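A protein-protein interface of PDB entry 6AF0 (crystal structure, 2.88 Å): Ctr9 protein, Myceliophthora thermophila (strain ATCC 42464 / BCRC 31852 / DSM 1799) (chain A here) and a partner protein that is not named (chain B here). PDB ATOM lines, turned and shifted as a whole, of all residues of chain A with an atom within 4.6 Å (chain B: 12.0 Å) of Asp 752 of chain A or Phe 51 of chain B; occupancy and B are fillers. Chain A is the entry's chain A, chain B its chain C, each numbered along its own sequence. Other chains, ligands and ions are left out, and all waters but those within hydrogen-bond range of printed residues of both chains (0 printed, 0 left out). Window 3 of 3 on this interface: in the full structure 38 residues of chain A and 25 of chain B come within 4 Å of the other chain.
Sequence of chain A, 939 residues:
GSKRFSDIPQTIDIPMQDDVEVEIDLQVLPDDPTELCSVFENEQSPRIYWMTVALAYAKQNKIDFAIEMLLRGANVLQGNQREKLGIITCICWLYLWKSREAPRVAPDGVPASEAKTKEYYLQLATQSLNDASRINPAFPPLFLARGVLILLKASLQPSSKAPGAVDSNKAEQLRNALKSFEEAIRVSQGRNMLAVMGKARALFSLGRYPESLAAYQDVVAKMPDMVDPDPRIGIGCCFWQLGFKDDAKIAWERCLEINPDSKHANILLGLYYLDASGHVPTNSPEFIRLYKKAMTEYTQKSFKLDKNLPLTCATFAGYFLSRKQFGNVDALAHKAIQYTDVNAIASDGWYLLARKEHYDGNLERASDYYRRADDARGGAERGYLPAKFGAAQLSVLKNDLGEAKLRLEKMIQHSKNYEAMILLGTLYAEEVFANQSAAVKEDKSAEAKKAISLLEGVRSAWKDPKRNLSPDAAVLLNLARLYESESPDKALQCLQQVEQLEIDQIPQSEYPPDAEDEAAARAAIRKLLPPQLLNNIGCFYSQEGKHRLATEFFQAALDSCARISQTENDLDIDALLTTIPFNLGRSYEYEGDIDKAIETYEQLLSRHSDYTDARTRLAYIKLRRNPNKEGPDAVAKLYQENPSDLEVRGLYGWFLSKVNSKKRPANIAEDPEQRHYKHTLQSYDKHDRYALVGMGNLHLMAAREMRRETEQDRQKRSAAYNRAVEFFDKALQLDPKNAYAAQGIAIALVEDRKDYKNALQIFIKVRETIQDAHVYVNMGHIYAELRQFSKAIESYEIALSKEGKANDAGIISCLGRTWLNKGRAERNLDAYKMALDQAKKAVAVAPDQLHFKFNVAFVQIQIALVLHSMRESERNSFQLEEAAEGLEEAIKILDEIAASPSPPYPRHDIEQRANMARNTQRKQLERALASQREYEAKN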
ATOM      1  N   SER A 718     -37.673 -24.775 -14.076  1.00  0.00           N
ATOM      2  CA  SER A 718     -36.802 -24.208 -15.107  1.00  0.00           C
ATOM      3  C   SER A 718     -36.120 -22.895 -14.635  1.00  0.00           C
ATOM      4  O   SER A 718     -35.097 -22.479 -15.168  1.00  0.00           O
ATOM      5  CB  SER A 718     -37.569 -23.970 -16.397  1.00  0.00           C
ATOM      6  OG  SER A 718     -36.656 -23.832 -17.470  1.00  0.00           O
ATOM      7  N   TYR A 721     -33.204 -24.475 -12.522  1.00  0.00           N
ATOM      8  CA  TYR A 721     -32.068 -24.784 -13.404  1.00  0.00           C
ATOM      9  C   TYR A 721     -31.283 -23.526 -13.743  1.00  0.00           C
ATOM     10  O   TYR A 721     -30.053 -23.541 -13.808  1.00  0.00           O
ATOM     11  CB  TYR A 721     -32.525 -25.449 -14.705  1.00  0.00           C
ATOM     12  CG  TYR A 721     -32.748 -26.944 -14.608  1.00  0.00           C
ATOM     13  CD1 TYR A 721     -33.398 -27.512 -13.507  1.00  0.00           C
ATOM     14  CD2 TYR A 721     -32.329 -27.793 -15.621  1.00  0.00           C
ATOM     15  CE1 TYR A 721     -33.607 -28.880 -13.425  1.00  0.00           C
ATOM     16  CE2 TYR A 721     -32.546 -29.155 -15.545  1.00  0.00           C
ATOM     17  CZ  TYR A 721     -33.183 -29.696 -14.445  1.00  0.00           C
ATOM     18  OH  TYR A 721     -33.393 -31.051 -14.358  1.00  0.00           O
ATOM     19  N   ASN A 722     -32.000 -22.435 -13.968  1.00  0.00           N
ATOM     20  CA  ASN A 722     -31.361 -21.155 -14.220  1.00  0.00           C
ATOM     21  C   ASN A 722     -30.350 -20.817 -13.111  1.00  0.00           C
ATOM     22  O   ASN A 722     -29.221 -20.422 -13.395  1.00  0.00           O
ATOM     23  CB  ASN A 722     -32.413 -20.050 -14.336  1.00  0.00           C
ATOM     24  CG  ASN A 722     -32.983 -19.910 -15.732  1.00  0.00           C
ATOM     25  OD1 ASN A 722     -33.409 -18.824 -16.100  1.00  0.00           O
ATOM     26  ND2 ASN A 722     -33.006 -20.986 -16.506  1.00  0.00           N
ATOM     27  N   VAL A 725     -27.261 -22.858 -13.287  1.00  0.00           N
ATOM     28  CA  VAL A 725     -26.386 -22.337 -14.327  1.00  0.00           C
ATOM     29  C   VAL A 725     -25.727 -21.011 -13.893  1.00  0.00           C
ATOM     30  O   VAL A 725     -24.593 -20.720 -14.285  1.00  0.00           O
ATOM     31  CB  VAL A 725     -27.143 -22.216 -15.658  1.00  0.00           C
ATOM     32  CG1 VAL A 725     -26.287 -21.560 -16.724  1.00  0.00           C
ATOM     33  CG2 VAL A 725     -27.572 -23.599 -16.132  1.00  0.00           C
ATOM     34  N   ALA A 748     -27.459 -29.441 -17.485  1.00  0.00           N
ATOM     35  CA  ALA A 748     -28.507 -28.447 -17.549  1.00  0.00           C
ATOM     36  C   ALA A 748     -29.048 -28.445 -18.975  1.00  0.00           C
ATOM     37  O   ALA A 748     -30.259 -28.402 -19.216  1.00  0.00           O
ATOM     38  CB  ALA A 748     -27.959 -27.082 -17.198  1.00  0.00           C
ATOM     39  N   LEU A 749     -28.134 -28.522 -19.924  1.00  0.00           N
ATOM     40  CA  LEU A 749     -28.526 -28.484 -21.311  1.00  0.00           C
ATOM     41  C   LEU A 749     -29.530 -29.586 -21.551  1.00  0.00           C
ATOM     42  O   LEU A 749     -30.685 -29.323 -21.888  1.00  0.00           O
ATOM     43  CB  LEU A 749     -27.307 -28.664 -22.222  1.00  0.00           C
ATOM     44  CG  LEU A 749     -27.000 -27.495 -23.137  1.00  0.00           C
ATOM     45  CD1 LEU A 749     -26.905 -26.214 -22.325  1.00  0.00           C
ATOM     46  CD2 LEU A 749     -25.697 -27.789 -23.858  1.00  0.00           C
ATOM     47  N   VAL A 750     -29.097 -30.818 -21.310  1.00  0.00           N
ATOM     48  CA  VAL A 750     -29.883 -31.962 -21.728  1.00  0.00           C
ATOM     49  C   VAL A 750     -31.280 -31.962 -21.100  1.00  0.00           C
ATOM     50  O   VAL A 750     -32.272 -32.271 -21.749  1.00  0.00           O
ATOM     51  CB  VAL A 750     -29.162 -33.282 -21.406  1.00  0.00           C
ATOM     52  CG1 VAL A 750     -29.006 -33.441 -19.910  1.00  0.00           C
ATOM     53  CG2 VAL A 750     -29.934 -34.464 -21.972  1.00  0.00           C
ATOM     54  N   GLU A 751     -31.352 -31.613 -19.833  1.00  0.00           N
ATOM     55  CA  GLU A 751     -32.593 -31.737 -19.099  1.00  0.00           C
ATOM     56  C   GLU A 751     -33.534 -30.573 -19.362  1.00  0.00           C
ATOM     57  O   GLU A 751     -34.716 -30.790 -19.611  1.00  0.00           O
ATOM     58  CB  GLU A 751     -32.300 -31.849 -17.613  1.00  0.00           C
ATOM     59  CG  GLU A 751     -31.481 -33.074 -17.262  1.00  0.00           C
ATOM     60  CD  GLU A 751     -31.311 -33.275 -15.776  1.00  0.00           C
ATOM     61  OE1 GLU A 751     -31.400 -32.285 -15.019  1.00  0.00           O
ATOM     62  OE2 GLU A 751     -31.067 -34.433 -15.377  1.00  0.00           O
ATOM     63  N   ASP A 752     -33.030 -29.340 -19.305  1.00  0.00           N
ATOM     64  CA  ASP A 752     -33.918 -28.188 -19.493  1.00  0.00           C
ATOM     65  C   ASP A 752     -34.238 -27.953 -20.946  1.00  0.00           C
ATOM     66  O   ASP A 752     -35.379 -27.691 -21.265  1.00  0.00           O
ATOM     67  CB  ASP A 752     -33.385 -26.895 -18.898  1.00  0.00           C
ATOM     68  CG  ASP A 752     -34.467 -25.825 -18.798  1.00  0.00           C
ATOM     69  OD1 ASP A 752     -34.933 -25.570 -17.665  1.00  0.00           O
ATOM     70  OD2 ASP A 752     -34.877 -25.269 -19.846  1.00  0.00           O
ATOM     71  N   ARG A 753     -33.239 -28.004 -21.815  1.00  0.00           N
ATOM     72  CA  ARG A 753     -33.487 -27.922 -23.262  1.00  0.00           C
ATOM     73  C   ARG A 753     -32.800 -29.042 -23.961  1.00  0.00           C
ATOM     74  O   ARG A 753     -31.585 -29.046 -24.085  1.00  0.00           O
ATOM     75  CB  ARG A 753     -33.011 -26.616 -23.897  1.00  0.00           C
ATOM     76  CG  ARG A 753     -32.162 -25.701 -23.029  1.00  0.00           C
ATOM     77  CD  ARG A 753     -33.010 -24.577 -22.440  1.00  0.00           C
ATOM     78  NE  ARG A 753     -32.501 -23.262 -22.824  1.00  0.00           N
ATOM     79  CZ  ARG A 753     -32.589 -22.737 -24.050  1.00  0.00           C
ATOM     80  NH1 ARG A 753     -33.170 -23.398 -25.056  1.00  0.00           N
ATOM     81  NH2 ARG A 753     -32.079 -21.532 -24.281  1.00  0.00           N
ATOM     82  N   LYS A 754     -33.579 -29.950 -24.508  1.00  0.00           N
ATOM     83  CA  LYS A 754     -33.045 -31.244 -24.865  1.00  0.00           C
ATOM     84  C   LYS A 754     -32.046 -31.036 -25.985  1.00  0.00           C
ATOM     85  O   LYS A 754     -32.289 -31.418 -27.122  1.00  0.00           O
ATOM     86  CB  LYS A 754     -34.151 -32.217 -25.278  1.00  0.00           C
ATOM     87  CG  LYS A 754     -35.541 -31.926 -24.749  1.00  0.00           C
ATOM     88  CD  LYS A 754     -35.756 -32.487 -23.359  1.00  0.00           C
ATOM     89  CE  LYS A 754     -37.047 -31.932 -22.778  1.00  0.00           C
ATOM     90  NZ  LYS A 754     -37.603 -32.812 -21.714  1.00  0.00           N
ATOM     91  N   SER B  42     -14.717 -21.966 -21.997  1.00  0.00           N
ATOM     92  CA  SER B  42     -15.361 -20.651 -22.005  1.00  0.00           C
ATOM     93  C   SER B  42     -16.434 -20.552 -23.098  1.00  0.00           C
ATOM     94  O   SER B  42     -17.378 -19.771 -22.967  1.00  0.00           O
ATOM     95  CB  SER B  42     -14.315 -19.546 -22.121  1.00  0.00           C
ATOM     96  OG  SER B  42     -13.333 -19.859 -23.085  1.00  0.00           O
ATOM     97  N   HIS B  43     -16.305 -21.368 -24.144  1.00  0.00           N
ATOM     98  CA  HIS B  43     -17.393 -21.548 -25.115  1.00  0.00           C
ATOM     99  C   HIS B  43     -18.648 -22.138 -24.458  1.00  0.00           C
ATOM    100  O   HIS B  43     -19.782 -21.850 -24.845  1.00  0.00           O
ATOM    101  CB  HIS B  43     -16.956 -22.438 -26.278  1.00  0.00           C
ATOM    102  CG  HIS B  43     -16.677 -23.856 -25.886  1.00  0.00           C
ATOM    103  ND1 HIS B  43     -15.496 -24.244 -25.293  1.00  0.00           N
ATOM    104  CD2 HIS B  43     -17.424 -24.980 -26.005  1.00  0.00           C
ATOM    105  CE1 HIS B  43     -15.528 -25.544 -25.060  1.00  0.00           C
ATOM    106  NE2 HIS B  43     -16.684 -26.016 -25.488  1.00  0.00           N
ATOM    107  N   VAL B  44     -18.431 -22.974 -23.462  1.00  0.00           N
ATOM    108  CA  VAL B  44     -19.521 -23.458 -22.651  1.00  0.00           C
ATOM    109  C   VAL B  44     -20.124 -22.274 -21.876  1.00  0.00           C
ATOM    110  O   VAL B  44     -21.322 -22.260 -21.599  1.00  0.00           O
ATOM    111  CB  VAL B  44     -19.041 -24.553 -21.693  1.00  0.00           C
ATOM    112  CG1 VAL B  44     -20.222 -25.186 -20.970  1.00  0.00           C
ATOM    113  CG2 VAL B  44     -18.252 -25.615 -22.455  1.00  0.00           C
ATOM    114  N   ARG B  45     -19.295 -21.283 -21.536  1.00  0.00           N
ATOM    115  CA  ARG B  45     -19.784 -20.070 -20.890  1.00  0.00           C
ATOM    116  C   ARG B  45     -20.758 -19.407 -21.834  1.00  0.00           C
ATOM    117  O   ARG B  45     -21.859 -19.015 -21.445  1.00  0.00           O
ATOM    118  CB  ARG B  45     -18.645 -19.110 -20.546  1.00  0.00           C
ATOM    119  CG  ARG B  45     -19.060 -18.017 -19.570  1.00  0.00           C
ATOM    120  CD  ARG B  45     -17.952 -17.669 -18.598  1.00  0.00           C
ATOM    121  NE  ARG B  45     -17.072 -16.601 -19.085  1.00  0.00           N
ATOM    122  CZ  ARG B  45     -15.866 -16.763 -19.642  1.00  0.00           C
ATOM    123  NH1 ARG B  45     -15.338 -17.969 -19.833  1.00  0.00           N
ATOM    124  NH2 ARG B  45     -15.174 -15.692 -20.016  1.00  0.00           N
ATOM    125  N   LYS B  46     -20.346 -19.308 -23.092  1.00  0.00           N
ATOM    126  CA  LYS B  46     -21.205 -18.789 -24.157  1.00  0.00           C
ATOM    127  C   LYS B  46     -22.593 -19.438 -24.175  1.00  0.00           C
ATOM    128  O   LYS B  46     -23.583 -18.743 -24.353  1.00  0.00           O
ATOM    129  CB  LYS B  46     -20.521 -18.935 -25.527  1.00  0.00           C
ATOM    130  CG  LYS B  46     -19.548 -17.806 -25.835  1.00  0.00           C
ATOM    131  CD  LYS B  46     -18.673 -18.089 -27.053  1.00  0.00           C
ATOM    132  CE  LYS B  46     -17.825 -16.883 -27.463  1.00  0.00           C
ATOM    133  NZ  LYS B  46     -18.355 -15.561 -27.020  1.00  0.00           N
ATOM    134  N   LEU B  47     -22.659 -20.755 -23.974  1.00  0.00           N
ATOM    135  CA  LEU B  47     -23.936 -21.503 -24.033  1.00  0.00           C
ATOM    136  C   LEU B  47     -24.655 -21.661 -22.701  1.00  0.00           C
ATOM    137  O   LEU B  47     -25.782 -22.164 -22.660  1.00  0.00           O
ATOM    138  CB  LEU B  47     -23.731 -22.886 -24.627  1.00  0.00           C
ATOM    139  CG  LEU B  47     -22.803 -22.926 -25.837  1.00  0.00           C
ATOM    140  CD1 LEU B  47     -22.827 -24.335 -26.411  1.00  0.00           C
ATOM    141  CD2 LEU B  47     -23.164 -21.865 -26.881  1.00  0.00           C
ATOM    142  N   ALA B  48     -23.996 -21.269 -21.618  1.00  0.00           N
ATOM    143  CA  ALA B  48     -24.673 -21.076 -20.354  1.00  0.00           C
ATOM    144  C   ALA B  48     -25.433 -19.759 -20.434  1.00  0.00           C
ATOM    145  O   ALA B  48     -26.485 -19.608 -19.825  1.00  0.00           O
ATOM    146  CB  ALA B  48     -23.669 -21.054 -19.218  1.00  0.00           C
ATOM    147  N   ALA B  49     -24.898 -18.820 -21.213  1.00  0.00           N
ATOM    148  CA  ALA B  49     -25.461 -17.471 -21.323  1.00  0.00           C
ATOM    149  C   ALA B  49     -26.907 -17.454 -21.832  1.00  0.00           C
ATOM    150  O   ALA B  49     -27.777 -16.845 -21.189  1.00  0.00           O
ATOM    151  CB  ALA B  49     -24.570 -16.584 -22.193  1.00  0.00           C
ATOM    152  N   PRO B  50     -27.178 -18.125 -22.974  1.00  0.00           N
ATOM    153  CA  PRO B  50     -28.559 -18.123 -23.444  1.00  0.00           C
ATOM    154  C   PRO B  50     -29.440 -18.949 -22.539  1.00  0.00           C
ATOM    155  O   PRO B  50     -30.655 -18.812 -22.566  1.00  0.00           O
ATOM    156  CB  PRO B  50     -28.464 -18.770 -24.824  1.00  0.00           C
ATOM    157  CG  PRO B  50     -27.299 -19.682 -24.710  1.00  0.00           C
ATOM    158  CD  PRO B  50     -26.317 -18.928 -23.857  1.00  0.00           C
ATOM    159  N   PHE B  51     -28.827 -19.807 -21.735  1.00  0.00           N
ATOM    160  CA  PHE B  51     -29.573 -20.514 -20.714  1.00  0.00           C
ATOM    161  C   PHE B  51     -30.331 -19.520 -19.825  1.00  0.00           C
ATOM    162  O   PHE B  51     -31.524 -19.700 -19.589  1.00  0.00           O
ATOM    163  CB  PHE B  51     -28.675 -21.436 -19.882  1.00  0.00           C
ATOM    164  CG  PHE B  51     -29.437 -22.506 -19.185  1.00  0.00           C
ATOM    165  CD1 PHE B  51     -30.150 -22.209 -18.023  1.00  0.00           C
ATOM    166  CD2 PHE B  51     -29.499 -23.786 -19.710  1.00  0.00           C
ATOM    167  CE1 PHE B  51     -30.883 -23.180 -17.380  1.00  0.00           C
ATOM    168  CE2 PHE B  51     -30.228 -24.762 -19.064  1.00  0.00           C
ATOM    169  CZ  PHE B  51     -30.924 -24.456 -17.899  1.00  0.00           C
ATOM    170  N   VAL B  52     -29.649 -18.469 -19.365  1.00  0.00           N
ATOM    171  CA  VAL B  52     -30.315 -17.386 -18.616  1.00  0.00           C
ATOM    172  C   VAL B  52     -30.133 -16.016 -19.286  1.00  0.00           C
ATOM    173  O   VAL B  52     -31.024 -15.161 -19.236  1.00  0.00           O
ATOM    174  CB  VAL B  52     -29.846 -17.333 -17.143  1.00  0.00           C
ATOM    175  CG1 VAL B  52     -28.503 -16.622 -17.010  1.00  0.00           C
ATOM    176  CG2 VAL B  52     -30.910 -16.666 -16.278  1.00  0.00           C
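Printed residues of chain B that touch a printed residue of chain A: Ala 48, Pro 50, Phe 51 and Val 52.
Of the 11 printed residues of chain A, 6 touch a printed residue of chain B.
The side-chain amide nitrogen (ND2) of Asn 722 of chain A sits at hydrogen-bond distance from the backbone carbonyl oxygen (O) of Ser 718 of chain A, 2.9 Å away.
OG of Ser 718 of chain A is in hydrogen-bond range of OD1 of Asp 752 of chain A (2.5 Å).
The side-chain hydroxyl (OH) of Tyr 721 of chain A is in hydrogen-bond range of the side-chain carboxylate (OE1) of Glu 751 of chain A (2.4 Å).
Asp 752 of chain A touches just one residue of chain B: Phe 51 (3.6 Å).
Of the printed residues of chain A, Phe 51 of chain B touches Tyr 721 (3.7 Å), Asn 722 (3.2 Å), Val 725 (3.5 Å), Ala 748 (3.6 Å) and Asp 752 (3.6 Å).
No residue of chain B comes within 4 Å of Ser 718 of chain A.
Tyr 721 of chain A touches just one residue of chain B: Phe 51.
Asn 722 of chain A touches just these residues of chain B: Phe 51 and Val 52.
Of chain B, only Ala 48 and Phe 51 come within 4 Å of Val 725 of chain A.
Leu 749 of chain A touches none of the printed residues of chain B.
Val 750 of chain A touches none of the printed residues of chain B.
No residue of chain B comes within 4 Å of Glu 751 of chain A.
No residue of chain B comes within 4 Å of Lys 754 of chain A.
Of the printed residues of chain A, Val 52 of chain B touches Asn 722.
Of the printed residues of chain A, Pro 50 of chain B touches Arg 753 (3.5 Å).
Of the printed residues of chain A, Ala 48 of chain B touches Val 725 (3.7 Å).
Ala 49 of chain B touches none of the printed residues of chain A.
Lys 46 of chain B touches none of the printed residues of chain A.
The nearest residue of chain A that does not touch Phe 51 of chain B is Arg 753 of chain A (4.4 Å).
The nearest printed residue of chain A that does not touch Ala 48 of chain B is Leu 749 of chain A (5.8 Å).
Among the printed residues, pairs that only touch across the chains: Tyr 721 of chain A with Phe 51 of chain B (3.7 Å), Asn 722 of chain A with Phe 51 of chain B (3.2 Å), Asn 722 of chain A with Val 52 of chain B (3.3 Å), Val 725 of chain A with Ala 48 of chain B (3.7 Å), Val 725 of chain A with Phe 51 of chain B (3.5 Å), Ala 748 of chain A with Phe 51 of chain B (3.6 Å), Asp 752 of chain A with Phe 51 of chain B (3.6 Å) and Arg 753 of chain A with Pro 50 of chain B (3.5 Å).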
